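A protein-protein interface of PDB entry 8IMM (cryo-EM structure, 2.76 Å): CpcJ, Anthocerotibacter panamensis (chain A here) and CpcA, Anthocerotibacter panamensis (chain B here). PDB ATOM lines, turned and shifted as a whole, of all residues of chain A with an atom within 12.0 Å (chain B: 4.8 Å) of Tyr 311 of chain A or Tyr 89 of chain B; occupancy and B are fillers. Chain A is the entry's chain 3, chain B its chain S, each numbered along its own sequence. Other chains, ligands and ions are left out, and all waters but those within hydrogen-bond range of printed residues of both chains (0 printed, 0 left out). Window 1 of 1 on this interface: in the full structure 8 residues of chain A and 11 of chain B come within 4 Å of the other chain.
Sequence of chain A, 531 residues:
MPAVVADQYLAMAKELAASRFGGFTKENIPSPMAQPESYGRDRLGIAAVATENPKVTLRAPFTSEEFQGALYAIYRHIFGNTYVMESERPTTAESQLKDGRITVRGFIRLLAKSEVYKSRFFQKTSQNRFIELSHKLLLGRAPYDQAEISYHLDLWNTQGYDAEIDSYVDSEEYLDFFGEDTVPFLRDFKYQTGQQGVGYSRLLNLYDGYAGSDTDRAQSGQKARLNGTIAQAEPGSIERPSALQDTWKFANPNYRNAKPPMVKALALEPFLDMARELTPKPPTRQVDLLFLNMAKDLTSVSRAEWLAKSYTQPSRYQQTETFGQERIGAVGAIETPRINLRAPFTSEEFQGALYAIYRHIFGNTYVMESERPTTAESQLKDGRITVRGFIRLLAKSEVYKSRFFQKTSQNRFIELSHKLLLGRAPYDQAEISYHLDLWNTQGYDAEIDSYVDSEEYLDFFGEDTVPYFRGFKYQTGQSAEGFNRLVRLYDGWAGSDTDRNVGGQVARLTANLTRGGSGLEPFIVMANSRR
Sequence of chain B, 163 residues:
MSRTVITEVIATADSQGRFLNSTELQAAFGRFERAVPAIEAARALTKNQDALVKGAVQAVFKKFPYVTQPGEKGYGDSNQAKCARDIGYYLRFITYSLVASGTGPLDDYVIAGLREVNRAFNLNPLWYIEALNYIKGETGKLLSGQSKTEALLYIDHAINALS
Printed residues of chain B within 4 Å of Leu 307 of chain A: Ser 78 (3.8 Å) and Ala 81 (3.6 Å).
Of the printed residues of chain B, Ala 308 of chain A touches Ala 81 (3.9 Å).
Of chain B, only Ser 78 (3.8 Å), Ala 81 (3.8 Å), Lys 82 (3.5 Å), Arg 85 (3.6 Å) and Tyr 89 (3.8 Å) come within 4 Å of Tyr 311 of chain A.
Printed residues of chain A within 4 Å of Ser 78 of chain B: Leu 307 (3.8 Å) and Tyr 311 (3.8 Å).
Of the printed residues of chain A, Ala 81 of chain B touches Ala 304 (3.98 Å), Leu 307 (3.6 Å), Ala 308 (3.9 Å) and Tyr 311 (3.8 Å).
Of the printed residues of chain A, Lys 82 of chain B touches Tyr 311 (3.5 Å).
Asp 86 of chain B touches none of the printed residues of chain A.
No residue of chain A comes within 4 Å of Gly 88 of chain B.
Of the printed residues of chain A, Tyr 89 of chain B touches Tyr 311.
No residue of chain A comes within 4 Å of Tyr 90 of chain B.
No residue of chain A comes within 4 Å of Leu 91 of chain B.
No residue of chain A comes within 4 Å of Arg 92 of chain B.
No residue of chain A comes within 4 Å of Phe 93 of chain B.
The nearest printed residue of chain B that does not touch Tyr 311 of chain A is Asp 86 of chain B (7.3 Å).
Among the printed residues, pairs that only touch across the chains: Ala 304 of chain A with Ala 81 of chain B (3.98 Å), Leu 307 of chain A with Ser 78 of chain B (3.8 Å), Leu 307 of chain A with Ala 81 of chain B (3.6 Å), Ala 308 of chain A with Ala 81 of chain B (3.9 Å), Tyr 311 of chain A with Ser 78 of chain B (3.8 Å), Tyr 311 of chain A with Ala 81 of chain B (3.8 Å), Tyr 311 of chain A with Lys 82 of chain B (3.5 Å), Tyr 311 of chain A with Arg 85 of chain B (3.6 Å) and Tyr 311 of chain A with Tyr 89 of chain B (3.8 Å).
Of the 18 printed residues of chain A, 4 touch a printed residue of chain B.
Hydrophobic or aromatic side chains of chain A that line the printed part of chain B: Leu 307 and Tyr 311.
Among the printed residues, no Asp or Glu carboxylate lies within 4 Å of a Lys or Arg side-chain nitrogen of the other chain.
The side-chain carboxylate (OD1) of Asp 86 of chain B lies within salt-bridge range of the guanidinium group (NH2) of Arg 85 of chain B (3.1 Å).
The backbone carbonyl oxygen (O) of Leu 307 of chain A is in hydrogen-bond range of the side-chain hydroxyl (OG) of Ser 310 of chain A.
The side-chain hydroxyl of Thr 312 of chain A is in hydrogen-bond range of the backbone carbonyl oxygen of Ala 308 of chain A, at 3.1 Å.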
ATOM      1  N   SER A 302     -22.024 -19.127  19.158  1.00  0.00           N
ATOM      2  CA  SER A 302     -20.941 -19.210  18.193  1.00  0.00           C
ATOM      3  C   SER A 302     -19.596 -19.301  18.903  1.00  0.00           C
ATOM      4  O   SER A 302     -19.439 -18.871  20.047  1.00  0.00           O
ATOM      5  CB  SER A 302     -20.954 -17.997  17.262  1.00  0.00           C
ATOM      6  OG  SER A 302     -20.456 -16.845  17.916  1.00  0.00           O
ATOM      7  N   ARG A 303     -18.615 -19.879  18.204  1.00  0.00           N
ATOM      8  CA  ARG A 303     -17.275 -19.978  18.774  1.00  0.00           C
ATOM      9  C   ARG A 303     -16.557 -18.637  18.757  1.00  0.00           C
ATOM     10  O   ARG A 303     -15.658 -18.408  19.572  1.00  0.00           O
ATOM     11  CB  ARG A 303     -16.452 -21.025  18.019  1.00  0.00           C
ATOM     12  CG  ARG A 303     -15.196 -21.477  18.757  1.00  0.00           C
ATOM     13  CD  ARG A 303     -14.533 -22.685  18.102  1.00  0.00           C
ATOM     14  NE  ARG A 303     -15.379 -23.877  18.118  1.00  0.00           N
ATOM     15  CZ  ARG A 303     -14.918 -25.125  18.137  1.00  0.00           C
ATOM     16  NH1 ARG A 303     -15.761 -26.144  18.149  1.00  0.00           N
ATOM     17  NH2 ARG A 303     -13.612 -25.358  18.148  1.00  0.00           N
ATOM     18  N   ALA A 304     -16.931 -17.744  17.839  1.00  0.00           N
ATOM     19  CA  ALA A 304     -16.194 -16.495  17.673  1.00  0.00           C
ATOM     20  C   ALA A 304     -16.283 -15.623  18.918  1.00  0.00           C
ATOM     21  O   ALA A 304     -15.260 -15.198  19.467  1.00  0.00           O
ATOM     22  CB  ALA A 304     -16.712 -15.738  16.453  1.00  0.00           C
ATOM     23  N   GLU A 305     -17.500 -15.350  19.393  1.00  0.00           N
ATOM     24  CA  GLU A 305     -17.599 -14.469  20.547  1.00  0.00           C
ATOM     25  C   GLU A 305     -17.116 -15.191  21.793  1.00  0.00           C
ATOM     26  O   GLU A 305     -16.638 -14.552  22.733  1.00  0.00           O
ATOM     27  CB  GLU A 305     -19.032 -13.968  20.742  1.00  0.00           C
ATOM     28  CG  GLU A 305     -20.050 -15.045  21.027  1.00  0.00           C
ATOM     29  CD  GLU A 305     -20.095 -15.345  22.516  1.00  0.00           C
ATOM     30  OE1 GLU A 305     -19.644 -14.480  23.297  1.00  0.00           O
ATOM     31  OE2 GLU A 305     -20.521 -16.445  22.910  1.00  0.00           O
ATOM     32  N   TRP A 306     -17.245 -16.520  21.817  1.00  0.00           N
ATOM     33  CA  TRP A 306     -16.666 -17.308  22.900  1.00  0.00           C
ATOM     34  C   TRP A 306     -15.174 -17.047  23.019  1.00  0.00           C
ATOM     35  O   TRP A 306     -14.661 -16.750  24.103  1.00  0.00           O
ATOM     36  CB  TRP A 306     -16.915 -18.795  22.656  1.00  0.00           C
ATOM     37  CG  TRP A 306     -16.267 -19.671  23.680  1.00  0.00           C
ATOM     38  CD1 TRP A 306     -15.313 -20.623  23.462  1.00  0.00           C
ATOM     39  CD2 TRP A 306     -16.539 -19.691  25.083  1.00  0.00           C
ATOM     40  NE1 TRP A 306     -14.964 -21.223  24.645  1.00  0.00           N
ATOM     41  CE2 TRP A 306     -15.707 -20.672  25.656  1.00  0.00           C
ATOM     42  CE3 TRP A 306     -17.405 -18.971  25.913  1.00  0.00           C
ATOM     43  CZ2 TRP A 306     -15.714 -20.949  27.020  1.00  0.00           C
ATOM     44  CZ3 TRP A 306     -17.411 -19.250  27.263  1.00  0.00           C
ATOM     45  CH2 TRP A 306     -16.571 -20.229  27.804  1.00  0.00           C
ATOM     46  N   LEU A 307     -14.461 -17.150  21.903  1.00  0.00           N
ATOM     47  CA  LEU A 307     -13.026 -16.914  21.931  1.00  0.00           C
ATOM     48  C   LEU A 307     -12.720 -15.463  22.268  1.00  0.00           C
ATOM     49  O   LEU A 307     -11.786 -15.180  23.027  1.00  0.00           O
ATOM     50  CB  LEU A 307     -12.413 -17.301  20.593  1.00  0.00           C
ATOM     51  CG  LEU A 307     -11.852 -18.716  20.515  1.00  0.00           C
ATOM     52  CD1 LEU A 307     -12.884 -19.733  20.973  1.00  0.00           C
ATOM     53  CD2 LEU A 307     -11.422 -18.999  19.105  1.00  0.00           C
ATOM     54  N   ALA A 308     -13.504 -14.531  21.725  1.00  0.00           N
ATOM     55  CA  ALA A 308     -13.268 -13.118  21.999  1.00  0.00           C
ATOM     56  C   ALA A 308     -13.403 -12.818  23.485  1.00  0.00           C
ATOM     57  O   ALA A 308     -12.576 -12.102  24.060  1.00  0.00           O
ATOM     58  CB  ALA A 308     -14.231 -12.257  21.186  1.00  0.00           C
ATOM     59  N   LYS A 309     -14.435 -13.363  24.129  1.00  0.00           N
ATOM     60  CA  LYS A 309     -14.601 -13.125  25.558  1.00  0.00           C
ATOM     61  C   LYS A 309     -13.558 -13.871  26.374  1.00  0.00           C
ATOM     62  O   LYS A 309     -13.166 -13.399  27.445  1.00  0.00           O
ATOM     63  CB  LYS A 309     -16.008 -13.513  26.019  1.00  0.00           C
ATOM     64  CG  LYS A 309     -16.337 -14.981  25.894  1.00  0.00           C
ATOM     65  CD  LYS A 309     -17.533 -15.361  26.743  1.00  0.00           C
ATOM     66  CE  LYS A 309     -17.195 -15.285  28.218  1.00  0.00           C
ATOM     67  NZ  LYS A 309     -16.602 -16.560  28.710  1.00  0.00           N
ATOM     68  N   SER A 310     -13.095 -15.026  25.896  1.00  0.00           N
ATOM     69  CA  SER A 310     -12.039 -15.731  26.612  1.00  0.00           C
ATOM     70  C   SER A 310     -10.725 -14.968  26.547  1.00  0.00           C
ATOM     71  O   SER A 310      -9.908 -15.045  27.468  1.00  0.00           O
ATOM     72  CB  SER A 310     -11.869 -17.136  26.046  1.00  0.00           C
ATOM     73  OG  SER A 310     -11.242 -17.095  24.781  1.00  0.00           O
ATOM     74  N   TYR A 311     -10.496 -14.235  25.457  1.00  0.00           N
ATOM     75  CA  TYR A 311      -9.230 -13.528  25.299  1.00  0.00           C
ATOM     76  C   TYR A 311      -9.167 -12.292  26.184  1.00  0.00           C
ATOM     77  O   TYR A 311      -8.079 -11.821  26.527  1.00  0.00           O
ATOM     78  CB  TYR A 311      -9.019 -13.140  23.840  1.00  0.00           C
ATOM     79  CG  TYR A 311      -8.768 -14.295  22.911  1.00  0.00           C
ATOM     80  CD1 TYR A 311      -8.508 -15.560  23.402  1.00  0.00           C
ATOM     81  CD2 TYR A 311      -8.789 -14.121  21.538  1.00  0.00           C
ATOM     82  CE1 TYR A 311      -8.282 -16.617  22.551  1.00  0.00           C
ATOM     83  CE2 TYR A 311      -8.563 -15.173  20.684  1.00  0.00           C
ATOM     84  CZ  TYR A 311      -8.305 -16.418  21.197  1.00  0.00           C
ATOM     85  OH  TYR A 311      -8.074 -17.479  20.359  1.00  0.00           O
ATOM     86  N   THR A 312     -10.317 -11.742  26.549  1.00  0.00           N
ATOM     87  CA  THR A 312     -10.370 -10.507  27.315  1.00  0.00           C
ATOM     88  C   THR A 312     -10.634 -10.761  28.797  1.00  0.00           C
ATOM     89  O   THR A 312     -10.776  -9.809  29.568  1.00  0.00           O
ATOM     90  CB  THR A 312     -11.443  -9.588  26.715  1.00  0.00           C
ATOM     91  OG1 THR A 312     -11.263  -9.535  25.298  1.00  0.00           O
ATOM     92  CG2 THR A 312     -11.300  -8.163  27.225  1.00  0.00           C
ATOM     93  N   GLN A 313     -10.700 -12.020  29.216  1.00  0.00           N
ATOM     94  CA  GLN A 313     -10.876 -12.314  30.622  1.00  0.00           C
ATOM     95  C   GLN A 313      -9.707 -11.750  31.419  1.00  0.00           C
ATOM     96  O   GLN A 313      -8.552 -11.871  31.009  1.00  0.00           O
ATOM     97  CB  GLN A 313     -10.976 -13.814  30.860  1.00  0.00           C
ATOM     98  CG  GLN A 313     -12.197 -14.449  30.243  1.00  0.00           C
ATOM     99  CD  GLN A 313     -13.481 -13.900  30.825  1.00  0.00           C
ATOM    100  OE1 GLN A 313     -14.217 -13.174  30.159  1.00  0.00           O
ATOM    101  NE2 GLN A 313     -13.752 -14.238  32.082  1.00  0.00           N
ATOM    102  N   PRO A 314      -9.982 -11.113  32.553  1.00  0.00           N
ATOM    103  CA  PRO A 314      -8.898 -10.543  33.347  1.00  0.00           C
ATOM    104  C   PRO A 314      -7.904 -11.603  33.768  1.00  0.00           C
ATOM    105  O   PRO A 314      -8.270 -12.701  34.184  1.00  0.00           O
ATOM    106  CB  PRO A 314      -9.624  -9.941  34.549  1.00  0.00           C
ATOM    107  CG  PRO A 314     -10.919 -10.616  34.590  1.00  0.00           C
ATOM    108  CD  PRO A 314     -11.287 -10.881  33.179  1.00  0.00           C
ATOM    109  N   SER A 315      -6.635 -11.257  33.661  1.00  0.00           N
ATOM    110  CA  SER A 315      -5.577 -12.182  33.996  1.00  0.00           C
ATOM    111  C   SER A 315      -5.535 -12.430  35.494  1.00  0.00           C
ATOM    112  O   SER A 315      -6.074 -11.656  36.284  1.00  0.00           O
ATOM    113  CB  SER A 315      -4.239 -11.643  33.517  1.00  0.00           C
ATOM    114  OG  SER A 315      -3.180 -12.336  34.129  1.00  0.00           O
ATOM    115  N   ARG A 316      -4.914 -13.543  35.883  1.00  0.00           N
ATOM    116  CA  ARG A 316      -4.780 -13.836  37.306  1.00  0.00           C
ATOM    117  C   ARG A 316      -3.589 -13.102  37.899  1.00  0.00           C
ATOM    118  O   ARG A 316      -3.585 -12.776  39.089  1.00  0.00           O
ATOM    119  CB  ARG A 316      -4.668 -15.340  37.532  1.00  0.00           C
ATOM    120  CG  ARG A 316      -3.333 -15.913  37.179  1.00  0.00           C
ATOM    121  CD  ARG A 316      -2.997 -17.106  38.023  1.00  0.00           C
ATOM    122  NE  ARG A 316      -2.091 -17.990  37.306  1.00  0.00           N
ATOM    123  CZ  ARG A 316      -0.794 -18.092  37.558  1.00  0.00           C
ATOM    124  NH1 ARG A 316      -0.251 -17.363  38.519  1.00  0.00           N
ATOM    125  NH2 ARG A 316      -0.043 -18.921  36.850  1.00  0.00           N
ATOM    126  N   TYR A 317      -2.567 -12.840  37.093  1.00  0.00           N
ATOM    127  CA  TYR A 317      -1.614 -11.792  37.422  1.00  0.00           C
ATOM    128  C   TYR A 317      -2.351 -10.470  37.339  1.00  0.00           C
ATOM    129  O   TYR A 317      -2.791 -10.072  36.256  1.00  0.00           O
ATOM    130  CB  TYR A 317      -0.443 -11.789  36.447  1.00  0.00           C
ATOM    131  CG  TYR A 317       0.190 -13.127  36.191  1.00  0.00           C
ATOM    132  CD1 TYR A 317       1.072 -13.683  37.094  1.00  0.00           C
ATOM    133  CD2 TYR A 317      -0.089 -13.829  35.038  1.00  0.00           C
ATOM    134  CE1 TYR A 317       1.652 -14.900  36.858  1.00  0.00           C
ATOM    135  CE2 TYR A 317       0.488 -15.042  34.792  1.00  0.00           C
ATOM    136  CZ  TYR A 317       1.359 -15.576  35.703  1.00  0.00           C
ATOM    137  OH  TYR A 317       1.930 -16.799  35.457  1.00  0.00           O
ATOM    138  N   GLN A 318      -2.529  -9.800  38.464  1.00  0.00           N
ATOM    139  CA  GLN A 318      -3.205  -8.514  38.459  1.00  0.00           C
ATOM    140  C   GLN A 318      -2.116  -7.451  38.446  1.00  0.00           C
ATOM    141  O   GLN A 318      -1.799  -6.828  39.457  1.00  0.00           O
ATOM    142  CB  GLN A 318      -4.135  -8.395  39.658  1.00  0.00           C
ATOM    143  CG  GLN A 318      -5.466  -9.133  39.512  1.00  0.00           C
ATOM    144  CD  GLN A 318      -6.241  -8.751  38.268  1.00  0.00           C
ATOM    145  OE1 GLN A 318      -5.864  -9.087  37.153  1.00  0.00           O
ATOM    146  NE2 GLN A 318      -7.349  -8.052  38.462  1.00  0.00           N
ATOM    147  N   GLN A 319      -1.526  -7.258  37.268  1.00  0.00           N
ATOM    148  CA  GLN A 319      -0.363  -6.404  37.107  1.00  0.00           C
ATOM    149  C   GLN A 319      -0.721  -5.220  36.228  1.00  0.00           C
ATOM    150  O   GLN A 319      -1.076  -5.399  35.060  1.00  0.00           O
ATOM    151  CB  GLN A 319       0.794  -7.176  36.485  1.00  0.00           C
ATOM    152  CG  GLN A 319       1.210  -8.363  37.274  1.00  0.00           C
ATOM    153  CD  GLN A 319       2.498  -8.942  36.798  1.00  0.00           C
ATOM    154  OE1 GLN A 319       3.038  -8.523  35.787  1.00  0.00           O
ATOM    155  NE2 GLN A 319       3.020  -9.903  37.534  1.00  0.00           N
ATOM    156  N   SER B  78      -9.842 -18.342  15.549  1.00  0.00           N
ATOM    157  CA  SER B  78      -8.907 -17.758  16.500  1.00  0.00           C
ATOM    158  C   SER B  78      -8.383 -16.426  15.998  1.00  0.00           C
ATOM    159  O   SER B  78      -8.307 -15.453  16.756  1.00  0.00           O
ATOM    160  CB  SER B  78      -7.747 -18.714  16.758  1.00  0.00           C
ATOM    161  OG  SER B  78      -8.212 -19.957  17.247  1.00  0.00           O
ATOM    162  N   ALA B  81     -11.140 -13.788  16.105  1.00  0.00           N
ATOM    163  CA  ALA B  81     -11.376 -13.422  17.493  1.00  0.00           C
ATOM    164  C   ALA B  81     -10.281 -12.504  18.011  1.00  0.00           C
ATOM    165  O   ALA B  81     -10.558 -11.542  18.733  1.00  0.00           O
ATOM    166  CB  ALA B  81     -11.472 -14.677  18.351  1.00  0.00           C
ATOM    167  N   LYS B  82      -9.030 -12.790  17.658  1.00  0.00           N
ATOM    168  CA  LYS B  82      -7.938 -11.903  18.020  1.00  0.00           C
ATOM    169  C   LYS B  82      -8.074 -10.553  17.347  1.00  0.00           C
ATOM    170  O   LYS B  82      -7.670  -9.537  17.912  1.00  0.00           O
ATOM    171  CB  LYS B  82      -6.609 -12.535  17.653  1.00  0.00           C
ATOM    172  CG  LYS B  82      -6.225 -13.689  18.529  1.00  0.00           C
ATOM    173  CD  LYS B  82      -4.968 -14.330  18.033  1.00  0.00           C
ATOM    174  CE  LYS B  82      -4.468 -15.368  18.996  1.00  0.00           C
ATOM    175  NZ  LYS B  82      -4.404 -14.838  20.374  1.00  0.00           N
ATOM    176  N   ARG B  85     -10.495  -8.736  19.381  1.00  0.00           N
ATOM    177  CA  ARG B  85      -9.842  -8.375  20.630  1.00  0.00           C
ATOM    178  C   ARG B  85      -8.937  -7.169  20.449  1.00  0.00           C
ATOM    179  O   ARG B  85      -8.893  -6.286  21.309  1.00  0.00           O
ATOM    180  CB  ARG B  85      -9.056  -9.564  21.157  1.00  0.00           C
ATOM    181  CG  ARG B  85      -8.423  -9.319  22.473  1.00  0.00           C
ATOM    182  CD  ARG B  85      -7.252 -10.221  22.652  1.00  0.00           C
ATOM    183  NE  ARG B  85      -6.339 -10.119  21.532  1.00  0.00           N
ATOM    184  CZ  ARG B  85      -5.234 -10.833  21.411  1.00  0.00           C
ATOM    185  NH1 ARG B  85      -4.898 -11.699  22.341  1.00  0.00           N
ATOM    186  NH2 ARG B  85      -4.464 -10.678  20.359  1.00  0.00           N
ATOM    187  N   ASP B  86      -8.206  -7.113  19.338  1.00  0.00           N
ATOM    188  CA  ASP B  86      -7.324  -5.981  19.080  1.00  0.00           C
ATOM    189  C   ASP B  86      -8.111  -4.696  18.878  1.00  0.00           C
ATOM    190  O   ASP B  86      -7.748  -3.642  19.414  1.00  0.00           O
ATOM    191  CB  ASP B  86      -6.470  -6.260  17.854  1.00  0.00           C
ATOM    192  CG  ASP B  86      -5.470  -7.341  18.083  1.00  0.00           C
ATOM    193  OD1 ASP B  86      -5.548  -8.007  19.128  1.00  0.00           O
ATOM    194  OD2 ASP B  86      -4.593  -7.519  17.225  1.00  0.00           O
ATOM    195  N   ILE B  87      -9.178  -4.753  18.085  1.00  0.00           N
ATOM    196  CA  ILE B  87      -9.951  -3.542  17.844  1.00  0.00           C
ATOM    197  C   ILE B  87     -10.626  -3.086  19.127  1.00  0.00           C
ATOM    198  O   ILE B  87     -10.728  -1.885  19.399  1.00  0.00           O
ATOM    199  CB  ILE B  87     -10.971  -3.762  16.714  1.00  0.00           C
ATOM    200  CG1 ILE B  87     -10.299  -4.347  15.480  1.00  0.00           C
ATOM    201  CG2 ILE B  87     -11.645  -2.462  16.356  1.00  0.00           C
ATOM    202  CD1 ILE B  87      -9.029  -3.680  15.103  1.00  0.00           C
ATOM    203  N   GLY B  88     -11.075  -4.031  19.946  1.00  0.00           N
ATOM    204  CA  GLY B  88     -11.602  -3.672  21.248  1.00  0.00           C
ATOM    205  C   GLY B  88     -10.549  -3.080  22.161  1.00  0.00           C
ATOM    206  O   GLY B  88     -10.835  -2.176  22.940  1.00  0.00           O
ATOM    207  N   TYR B  89      -9.320  -3.580  22.079  1.00  0.00           N
ATOM    208  CA  TYR B  89      -8.228  -2.982  22.829  1.00  0.00           C
ATOM    209  C   TYR B  89      -8.047  -1.529  22.436  1.00  0.00           C
ATOM    210  O   TYR B  89      -7.977  -0.639  23.291  1.00  0.00           O
ATOM    211  CB  TYR B  89      -6.937  -3.748  22.576  1.00  0.00           C
ATOM    212  CG  TYR B  89      -6.803  -5.030  23.346  1.00  0.00           C
ATOM    213  CD1 TYR B  89      -7.726  -5.383  24.301  1.00  0.00           C
ATOM    214  CD2 TYR B  89      -5.739  -5.872  23.129  1.00  0.00           C
ATOM    215  CE1 TYR B  89      -7.600  -6.536  25.000  1.00  0.00           C
ATOM    216  CE2 TYR B  89      -5.602  -7.027  23.826  1.00  0.00           C
ATOM    217  CZ  TYR B  89      -6.536  -7.356  24.763  1.00  0.00           C
ATOM    218  OH  TYR B  89      -6.408  -8.522  25.469  1.00  0.00           O
ATOM    219  N   TYR B  90      -7.969  -1.275  21.135  1.00  0.00           N
ATOM    220  CA  TYR B  90      -7.758   0.084  20.659  1.00  0.00           C
ATOM    221  C   TYR B  90      -8.887   0.994  21.107  1.00  0.00           C
ATOM    222  O   TYR B  90      -8.649   2.106  21.582  1.00  0.00           O
ATOM    223  CB  TYR B  90      -7.635   0.096  19.144  1.00  0.00           C
ATOM    224  CG  TYR B  90      -6.258  -0.210  18.647  1.00  0.00           C
ATOM    225  CD1 TYR B  90      -5.331   0.786  18.464  1.00  0.00           C
ATOM    226  CD2 TYR B  90      -5.891  -1.499  18.354  1.00  0.00           C
ATOM    227  CE1 TYR B  90      -4.082   0.505  18.004  1.00  0.00           C
ATOM    228  CE2 TYR B  90      -4.649  -1.793  17.901  1.00  0.00           C
ATOM    229  CZ  TYR B  90      -3.744  -0.792  17.730  1.00  0.00           C
ATOM    230  OH  TYR B  90      -2.495  -1.104  17.268  1.00  0.00           O
ATOM    231  N   LEU B  91     -10.127   0.532  20.976  1.00  0.00           N
ATOM    232  CA  LEU B  91     -11.261   1.341  21.399  1.00  0.00           C
ATOM    233  C   LEU B  91     -11.230   1.591  22.899  1.00  0.00           C
ATOM    234  O   LEU B  91     -11.524   2.701  23.360  1.00  0.00           O
ATOM    235  CB  LEU B  91     -12.556   0.655  20.990  1.00  0.00           C
ATOM    236  CG  LEU B  91     -13.796   1.505  20.772  1.00  0.00           C
ATOM    237  CD1 LEU B  91     -13.496   2.551  19.748  1.00  0.00           C
ATOM    238  CD2 LEU B  91     -14.920   0.618  20.303  1.00  0.00           C
ATOM    239  N   ARG B  92     -10.878   0.568  23.677  1.00  0.00           N
ATOM    240  CA  ARG B  92     -10.812   0.702  25.125  1.00  0.00           C
ATOM    241  C   ARG B  92      -9.825   1.774  25.523  1.00  0.00           C
ATOM    242  O   ARG B  92     -10.127   2.642  26.348  1.00  0.00           O
ATOM    243  CB  ARG B  92     -10.407  -0.630  25.738  1.00  0.00           C
ATOM    244  CG  ARG B  92     -10.891  -0.855  27.124  1.00  0.00           C
ATOM    245  CD  ARG B  92     -10.613  -2.261  27.563  1.00  0.00           C
ATOM    246  NE  ARG B  92      -9.308  -2.393  28.185  1.00  0.00           N
ATOM    247  CZ  ARG B  92      -8.449  -3.354  27.894  1.00  0.00           C
ATOM    248  NH1 ARG B  92      -8.770  -4.257  26.996  1.00  0.00           N
ATOM    249  NH2 ARG B  92      -7.280  -3.416  28.498  1.00  0.00           N
ATOM    250  N   PHE B  93      -8.645   1.742  24.929  1.00  0.00           N
ATOM    251  CA  PHE B  93      -7.631   2.716  25.275  1.00  0.00           C
ATOM    252  C   PHE B  93      -7.911   4.082  24.688  1.00  0.00           C
ATOM    253  O   PHE B  93      -7.470   5.083  25.255  1.00  0.00           O
ATOM    254  CB  PHE B  93      -6.272   2.203  24.853  1.00  0.00           C
ATOM    255  CG  PHE B  93      -5.825   1.036  25.650  1.00  0.00           C
ATOM    256  CD1 PHE B  93      -5.576   1.164  26.991  1.00  0.00           C
ATOM    257  CD2 PHE B  93      -5.698  -0.198  25.074  1.00  0.00           C
ATOM    258  CE1 PHE B  93      -5.186   0.090  27.724  1.00  0.00           C
ATOM    259  CE2 PHE B  93      -5.316  -1.266  25.802  1.00  0.00           C
ATOM    260  CZ  PHE B  93      -5.049  -1.128  27.126  1.00  0.00           C
